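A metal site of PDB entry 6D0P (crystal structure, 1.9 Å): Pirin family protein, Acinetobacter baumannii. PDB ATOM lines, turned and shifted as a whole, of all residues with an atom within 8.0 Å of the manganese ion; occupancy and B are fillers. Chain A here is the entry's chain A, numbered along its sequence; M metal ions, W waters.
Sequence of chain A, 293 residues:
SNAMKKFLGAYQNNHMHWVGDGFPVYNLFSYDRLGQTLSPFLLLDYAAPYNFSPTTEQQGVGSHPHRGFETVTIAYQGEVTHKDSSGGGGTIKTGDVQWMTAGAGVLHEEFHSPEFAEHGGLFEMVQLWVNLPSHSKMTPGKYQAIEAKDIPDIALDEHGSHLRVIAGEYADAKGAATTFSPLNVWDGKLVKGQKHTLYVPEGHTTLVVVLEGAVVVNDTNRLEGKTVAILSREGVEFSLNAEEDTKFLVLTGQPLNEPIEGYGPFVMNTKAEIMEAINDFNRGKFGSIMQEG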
ATOM      1  N   VAL A  19     -19.633  15.420   8.071  1.00  0.00           N
ATOM      2  CA  VAL A  19     -20.807  15.313   8.910  1.00  0.00           C
ATOM      3  C   VAL A  19     -21.807  14.521   8.062  1.00  0.00           C
ATOM      4  O   VAL A  19     -22.292  15.011   7.021  1.00  0.00           O
ATOM      5  CB  VAL A  19     -21.321  16.693   9.363  1.00  0.00           C
ATOM      6  CG1 VAL A  19     -22.639  16.586  10.117  1.00  0.00           C
ATOM      7  CG2 VAL A  19     -20.281  17.409  10.210  1.00  0.00           C
ATOM      8  N   VAL A  61     -27.231  13.910   7.015  1.00  0.00           N
ATOM      9  CA  VAL A  61     -27.058  13.300   8.310  1.00  0.00           C
ATOM     10  C   VAL A  61     -28.426  12.880   8.852  1.00  0.00           C
ATOM     11  O   VAL A  61     -29.412  13.609   8.755  1.00  0.00           O
ATOM     12  CB  VAL A  61     -26.301  14.278   9.250  1.00  0.00           C
ATOM     13  CG1 VAL A  61     -27.160  15.471   9.615  1.00  0.00           C
ATOM     14  CG2 VAL A  61     -25.789  13.586  10.496  1.00  0.00           C
ATOM     15  N   GLY A  62     -28.462  11.688   9.418  1.00  0.00           N
ATOM     16  CA  GLY A  62     -29.655  11.143   9.987  1.00  0.00           C
ATOM     17  C   GLY A  62     -29.977  11.765  11.343  1.00  0.00           C
ATOM     18  O   GLY A  62     -29.272  12.658  11.851  1.00  0.00           O
ATOM     19  N   SER A  63     -31.079  11.250  11.881  1.00  0.00           N
ATOM     20  CA  SER A  63     -31.717  11.683  13.118  1.00  0.00           C
ATOM     21  C   SER A  63     -30.672  11.911  14.227  1.00  0.00           C
ATOM     22  O   SER A  63     -29.922  11.037  14.558  1.00  0.00           O
ATOM     23  CB  SER A  63     -32.735  10.678  13.549  1.00  0.00           C
ATOM     24  OG  SER A  63     -33.392  11.137  14.701  1.00  0.00           O
ATOM     25  N   HIS A  64     -30.661  13.113  14.787  1.00  0.00           N
ATOM     26  CA  HIS A  64     -29.760  13.462  15.863  1.00  0.00           C
ATOM     27  C   HIS A  64     -30.431  14.546  16.717  1.00  0.00           C
ATOM     28  O   HIS A  64     -31.260  15.305  16.231  1.00  0.00           O
ATOM     29  CB  HIS A  64     -28.397  13.947  15.349  1.00  0.00           C
ATOM     30  CG  HIS A  64     -28.481  15.178  14.520  1.00  0.00           C
ATOM     31  ND1 HIS A  64     -28.773  15.124  13.173  1.00  0.00           N
ATOM     32  CD2 HIS A  64     -28.300  16.488  14.818  1.00  0.00           C
ATOM     33  CE1 HIS A  64     -28.774  16.351  12.678  1.00  0.00           C
ATOM     34  NE2 HIS A  64     -28.496  17.206  13.670  1.00  0.00           N
ATOM     35  N   PRO A  65     -30.078  14.606  17.987  1.00  0.00           N
ATOM     36  CA  PRO A  65     -30.658  15.574  18.876  1.00  0.00           C
ATOM     37  C   PRO A  65     -29.835  16.850  19.065  1.00  0.00           C
ATOM     38  O   PRO A  65     -28.621  16.866  18.772  1.00  0.00           O
ATOM     39  CB  PRO A  65     -30.723  14.832  20.207  1.00  0.00           C
ATOM     40  CG  PRO A  65     -29.496  13.969  20.184  1.00  0.00           C
ATOM     41  CD  PRO A  65     -29.374  13.554  18.739  1.00  0.00           C
ATOM     42  N   HIS A  66     -30.519  17.887  19.546  1.00  0.00           N
ATOM     43  CA  HIS A  66     -29.883  19.127  19.990  1.00  0.00           C
ATOM     44  C   HIS A  66     -30.648  19.639  21.208  1.00  0.00           C
ATOM     45  O   HIS A  66     -31.899  19.506  21.260  1.00  0.00           O
ATOM     46  CB  HIS A  66     -29.893  20.249  18.930  1.00  0.00           C
ATOM     47  CG  HIS A  66     -29.136  19.965  17.684  1.00  0.00           C
ATOM     48  ND1 HIS A  66     -27.761  19.809  17.688  1.00  0.00           N
ATOM     49  CD2 HIS A  66     -29.535  19.897  16.397  1.00  0.00           C
ATOM     50  CE1 HIS A  66     -27.351  19.603  16.438  1.00  0.00           C
ATOM     51  NE2 HIS A  66     -28.427  19.675  15.622  1.00  0.00           N
ATOM     52  N   PHE A  69     -29.271  25.377  22.557  1.00  0.00           N
ATOM     53  CA  PHE A  69     -28.701  26.407  21.723  1.00  0.00           C
ATOM     54  C   PHE A  69     -29.459  26.471  20.401  1.00  0.00           C
ATOM     55  O   PHE A  69     -30.519  25.831  20.241  1.00  0.00           O
ATOM     56  CB  PHE A  69     -27.192  26.133  21.541  1.00  0.00           C
ATOM     57  CG  PHE A  69     -26.913  24.819  20.875  1.00  0.00           C
ATOM     58  CD1 PHE A  69     -26.917  23.646  21.608  1.00  0.00           C
ATOM     59  CD2 PHE A  69     -26.649  24.762  19.525  1.00  0.00           C
ATOM     60  CE1 PHE A  69     -26.659  22.426  20.997  1.00  0.00           C
ATOM     61  CE2 PHE A  69     -26.402  23.537  18.919  1.00  0.00           C
ATOM     62  CZ  PHE A  69     -26.415  22.378  19.647  1.00  0.00           C
ATOM     63  N   THR A  71     -29.144  26.545  15.969  1.00  0.00           N
ATOM     64  CA  THR A  71     -28.331  26.242  14.787  1.00  0.00           C
ATOM     65  C   THR A  71     -28.824  27.117  13.650  1.00  0.00           C
ATOM     66  O   THR A  71     -30.050  27.253  13.417  1.00  0.00           O
ATOM     67  CB  THR A  71     -28.316  24.747  14.386  1.00  0.00           C
ATOM     68  OG1 THR A  71     -29.621  24.363  13.948  1.00  0.00           O
ATOM     69  CG2 THR A  71     -27.888  23.857  15.533  1.00  0.00           C
ATOM     70  N   THR A  73     -28.455  27.669   9.644  1.00  0.00           N
ATOM     71  CA  THR A  73     -27.985  27.067   8.401  1.00  0.00           C
ATOM     72  C   THR A  73     -28.179  28.096   7.283  1.00  0.00           C
ATOM     73  O   THR A  73     -29.309  28.593   7.074  1.00  0.00           O
ATOM     74  CB  THR A  73     -28.706  25.749   8.128  1.00  0.00           C
ATOM     75  OG1 THR A  73     -28.510  24.889   9.258  1.00  0.00           O
ATOM     76  CG2 THR A  73     -28.209  25.043   6.887  1.00  0.00           C
ATOM     77  N   HIS A  82     -34.707  19.717   5.947  1.00  0.00           N
ATOM     78  CA  HIS A  82     -34.598  19.244   7.313  1.00  0.00           C
ATOM     79  C   HIS A  82     -35.997  18.823   7.773  1.00  0.00           C
ATOM     80  O   HIS A  82     -36.985  19.346   7.278  1.00  0.00           O
ATOM     81  CB  HIS A  82     -33.947  20.284   8.228  1.00  0.00           C
ATOM     82  CG  HIS A  82     -34.613  21.619   8.200  1.00  0.00           C
ATOM     83  ND1 HIS A  82     -35.506  22.020   9.169  1.00  0.00           N
ATOM     84  CD2 HIS A  82     -34.578  22.616   7.278  1.00  0.00           C
ATOM     85  CE1 HIS A  82     -35.974  23.210   8.857  1.00  0.00           C
ATOM     86  NE2 HIS A  82     -35.416  23.610   7.704  1.00  0.00           N
ATOM     87  N   MET A 100     -32.798  28.017  13.673  1.00  0.00           N
ATOM     88  CA  MET A 100     -33.559  27.087  14.498  1.00  0.00           C
ATOM     89  C   MET A 100     -33.123  27.118  15.930  1.00  0.00           C
ATOM     90  O   MET A 100     -31.920  26.947  16.255  1.00  0.00           O
ATOM     91  CB  MET A 100     -33.365  25.650  13.999  1.00  0.00           C
ATOM     92  CG  MET A 100     -34.202  24.678  14.838  1.00  0.00           C
ATOM     93  SD  MET A 100     -33.803  22.787  14.334  1.00  0.00           S
ATOM     94  CE  MET A 100     -32.094  22.649  15.248  1.00  0.00           C
ATOM     95  N   VAL A 106     -34.857  19.116  20.254  1.00  0.00           N
ATOM     96  CA  VAL A 106     -35.320  18.764  18.939  1.00  0.00           C
ATOM     97  C   VAL A 106     -34.568  17.499  18.537  1.00  0.00           C
ATOM     98  O   VAL A 106     -33.403  17.281  18.932  1.00  0.00           O
ATOM     99  CB  VAL A 106     -35.092  19.904  17.916  1.00  0.00           C
ATOM    100  CG1 VAL A 106     -33.612  20.162  17.701  1.00  0.00           C
ATOM    101  CG2 VAL A 106     -35.742  19.626  16.576  1.00  0.00           C
ATOM    102  N   LEU A 107     -35.240  16.683  17.734  1.00  0.00           N
ATOM    103  CA  LEU A 107     -34.633  15.522  17.093  1.00  0.00           C
ATOM    104  C   LEU A 107     -34.880  15.689  15.583  1.00  0.00           C
ATOM    105  O   LEU A 107     -36.063  15.721  15.162  1.00  0.00           O
ATOM    106  CB  LEU A 107     -35.272  14.241  17.629  1.00  0.00           C
ATOM    107  CG  LEU A 107     -34.620  12.950  17.172  1.00  0.00           C
ATOM    108  CD1 LEU A 107     -33.265  12.764  17.843  1.00  0.00           C
ATOM    109  CD2 LEU A 107     -35.518  11.760  17.468  1.00  0.00           C
ATOM    110  N   HIS A 108     -33.810  15.824  14.794  1.00  0.00           N
ATOM    111  CA  HIS A 108     -34.015  16.112  13.383  1.00  0.00           C
ATOM    112  C   HIS A 108     -32.945  15.478  12.506  1.00  0.00           C
ATOM    113  O   HIS A 108     -31.895  14.999  12.960  1.00  0.00           O
ATOM    114  CB  HIS A 108     -34.164  17.631  13.194  1.00  0.00           C
ATOM    115  CG  HIS A 108     -32.906  18.428  13.191  1.00  0.00           C
ATOM    116  ND1 HIS A 108     -32.832  19.654  12.558  1.00  0.00           N
ATOM    117  CD2 HIS A 108     -31.667  18.176  13.656  1.00  0.00           C
ATOM    118  CE1 HIS A 108     -31.595  20.120  12.691  1.00  0.00           C
ATOM    119  NE2 HIS A 108     -30.873  19.234  13.346  1.00  0.00           N
ATOM    120  N   GLU A 109     -33.260  15.482  11.214  1.00  0.00           N
ATOM    121  CA  GLU A 109     -32.382  15.052  10.174  1.00  0.00           C
ATOM    122  C   GLU A 109     -32.198  16.231   9.212  1.00  0.00           C
ATOM    123  O   GLU A 109     -33.081  17.083   9.087  1.00  0.00           O
ATOM    124  CB  GLU A 109     -32.939  13.829   9.446  1.00  0.00           C
ATOM    125  CG  GLU A 109     -34.260  14.114   8.773  1.00  0.00           C
ATOM    126  CD  GLU A 109     -34.920  12.910   8.128  1.00  0.00           C
ATOM    127  OE1 GLU A 109     -35.597  13.101   7.078  1.00  0.00           O
ATOM    128  OE2 GLU A 109     -34.763  11.791   8.670  1.00  0.00           O
ATOM    129  N   GLU A 110     -31.039  16.272   8.557  1.00  0.00           N
ATOM    130  CA  GLU A 110     -30.667  17.315   7.606  1.00  0.00           C
ATOM    131  C   GLU A 110     -30.033  16.627   6.400  1.00  0.00           C
ATOM    132  O   GLU A 110     -29.033  15.919   6.525  1.00  0.00           O
ATOM    133  CB  GLU A 110     -29.690  18.329   8.238  1.00  0.00           C
ATOM    134  CG  GLU A 110     -30.252  19.069   9.448  1.00  0.00           C
ATOM    135  CD  GLU A 110     -29.247  19.837  10.319  1.00  0.00           C
ATOM    136  OE1 GLU A 110     -28.627  19.226  11.256  1.00  0.00           O
ATOM    137  OE2 GLU A 110     -29.119  21.064  10.101  1.00  0.00           O
ATOM    138  N   GLN A 127     -22.955  26.261   8.664  1.00  0.00           N
ATOM    139  CA  GLN A 127     -23.766  26.007   9.856  1.00  0.00           C
ATOM    140  C   GLN A 127     -23.064  26.651  11.067  1.00  0.00           C
ATOM    141  O   GLN A 127     -21.871  26.381  11.339  1.00  0.00           O
ATOM    142  CB  GLN A 127     -24.109  24.533  10.128  1.00  0.00           C
ATOM    143  CG  GLN A 127     -25.019  24.398  11.358  1.00  0.00           C
ATOM    144  CD  GLN A 127     -25.721  23.058  11.513  1.00  0.00           C
ATOM    145  OE1 GLN A 127     -25.411  22.288  12.438  1.00  0.00           O
ATOM    146  NE2 GLN A 127     -26.664  22.773  10.613  1.00  0.00           N
ATOM    147  N   TRP A 129     -23.553  27.545  15.184  1.00  0.00           N
ATOM    148  CA  TRP A 129     -24.254  27.316  16.433  1.00  0.00           C
ATOM    149  C   TRP A 129     -24.137  28.589  17.285  1.00  0.00           C
ATOM    150  O   TRP A 129     -23.027  29.099  17.437  1.00  0.00           O
ATOM    151  CB  TRP A 129     -23.673  26.140  17.171  1.00  0.00           C
ATOM    152  CG  TRP A 129     -23.855  24.798  16.538  1.00  0.00           C
ATOM    153  CD1 TRP A 129     -24.288  24.499  15.277  1.00  0.00           C
ATOM    154  CD2 TRP A 129     -23.491  23.546  17.146  1.00  0.00           C
ATOM    155  NE1 TRP A 129     -24.292  23.151  15.097  1.00  0.00           N
ATOM    156  CE2 TRP A 129     -23.808  22.533  16.214  1.00  0.00           C
ATOM    157  CE3 TRP A 129     -23.016  23.188  18.413  1.00  0.00           C
ATOM    158  CZ2 TRP A 129     -23.607  21.194  16.506  1.00  0.00           C
ATOM    159  CZ3 TRP A 129     -22.826  21.857  18.709  1.00  0.00           C
ATOM    160  CH2 TRP A 129     -23.096  20.873  17.758  1.00  0.00           C
ATOM    161  N   PRO A 265     -24.038  16.985  20.816  1.00  0.00           N
ATOM    162  CA  PRO A 265     -24.942  18.027  20.333  1.00  0.00           C
ATOM    163  C   PRO A 265     -25.750  18.723  21.451  1.00  0.00           C
ATOM    164  O   PRO A 265     -26.800  19.315  21.179  1.00  0.00           O
ATOM    165  CB  PRO A 265     -25.801  17.227  19.370  1.00  0.00           C
ATOM    166  CG  PRO A 265     -25.992  15.922  20.092  1.00  0.00           C
ATOM    167  CD  PRO A 265     -24.710  15.688  20.848  1.00  0.00           C
HETATM  168 MN    MN M   1     -28.615  19.345  13.470  1.00  0.00          MN
HETATM  169  O   HOH W   1     -28.819  21.721  12.842  1.00  0.00           O
HETATM  170  O   HOH W   2     -26.462  19.854  13.226  1.00  0.00           O
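Water W1 lies within hydrogen-bond range of the side-chain carboxylate (OE2) of Glu 110 (2.8 Å), the side-chain hydroxyl (OG1) of Thr 71 (3.0 Å) and the side-chain amide nitrogen (NE2) of Gln 127 (3.3 Å).
A ring nitrogen (NE2) of His 64 binds the manganese ion, at 2.2 Å.
A ring nitrogen (NE2) of His 66 is bound to the manganese ion.
The side-chain carboxylate (OE1) of Glu 110 binds the manganese ion, at 2.2 Å.
The manganese ion is bound by water W2 (2.2 Å).
NE2 of His 108 is bound to the manganese ion (2.3 Å).
Water W1 is bound to the manganese ion (2.5 Å).
ND1 of His 64 is in hydrogen-bond range of O of Gly 62.
N of His 66 sits at hydrogen-bond distance from O of Val 106.
OE2 of Glu 110 lies within hydrogen-bond range of NE2 of Gln 127, at 3.0 Å.
The backbone NH (N) of Val 61 lies within hydrogen-bond range of the backbone carbonyl oxygen (O) of Glu 110, at 2.7 Å.
ND1 of His 108 is in hydrogen-bond range of SD of Met 100 (3.7 Å).
Of the 20 residues printed, 4 come within 4 Å of the manganese ion.
Along chain A the residues within 4 Å of the manganese ion span positions 64 to 110.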
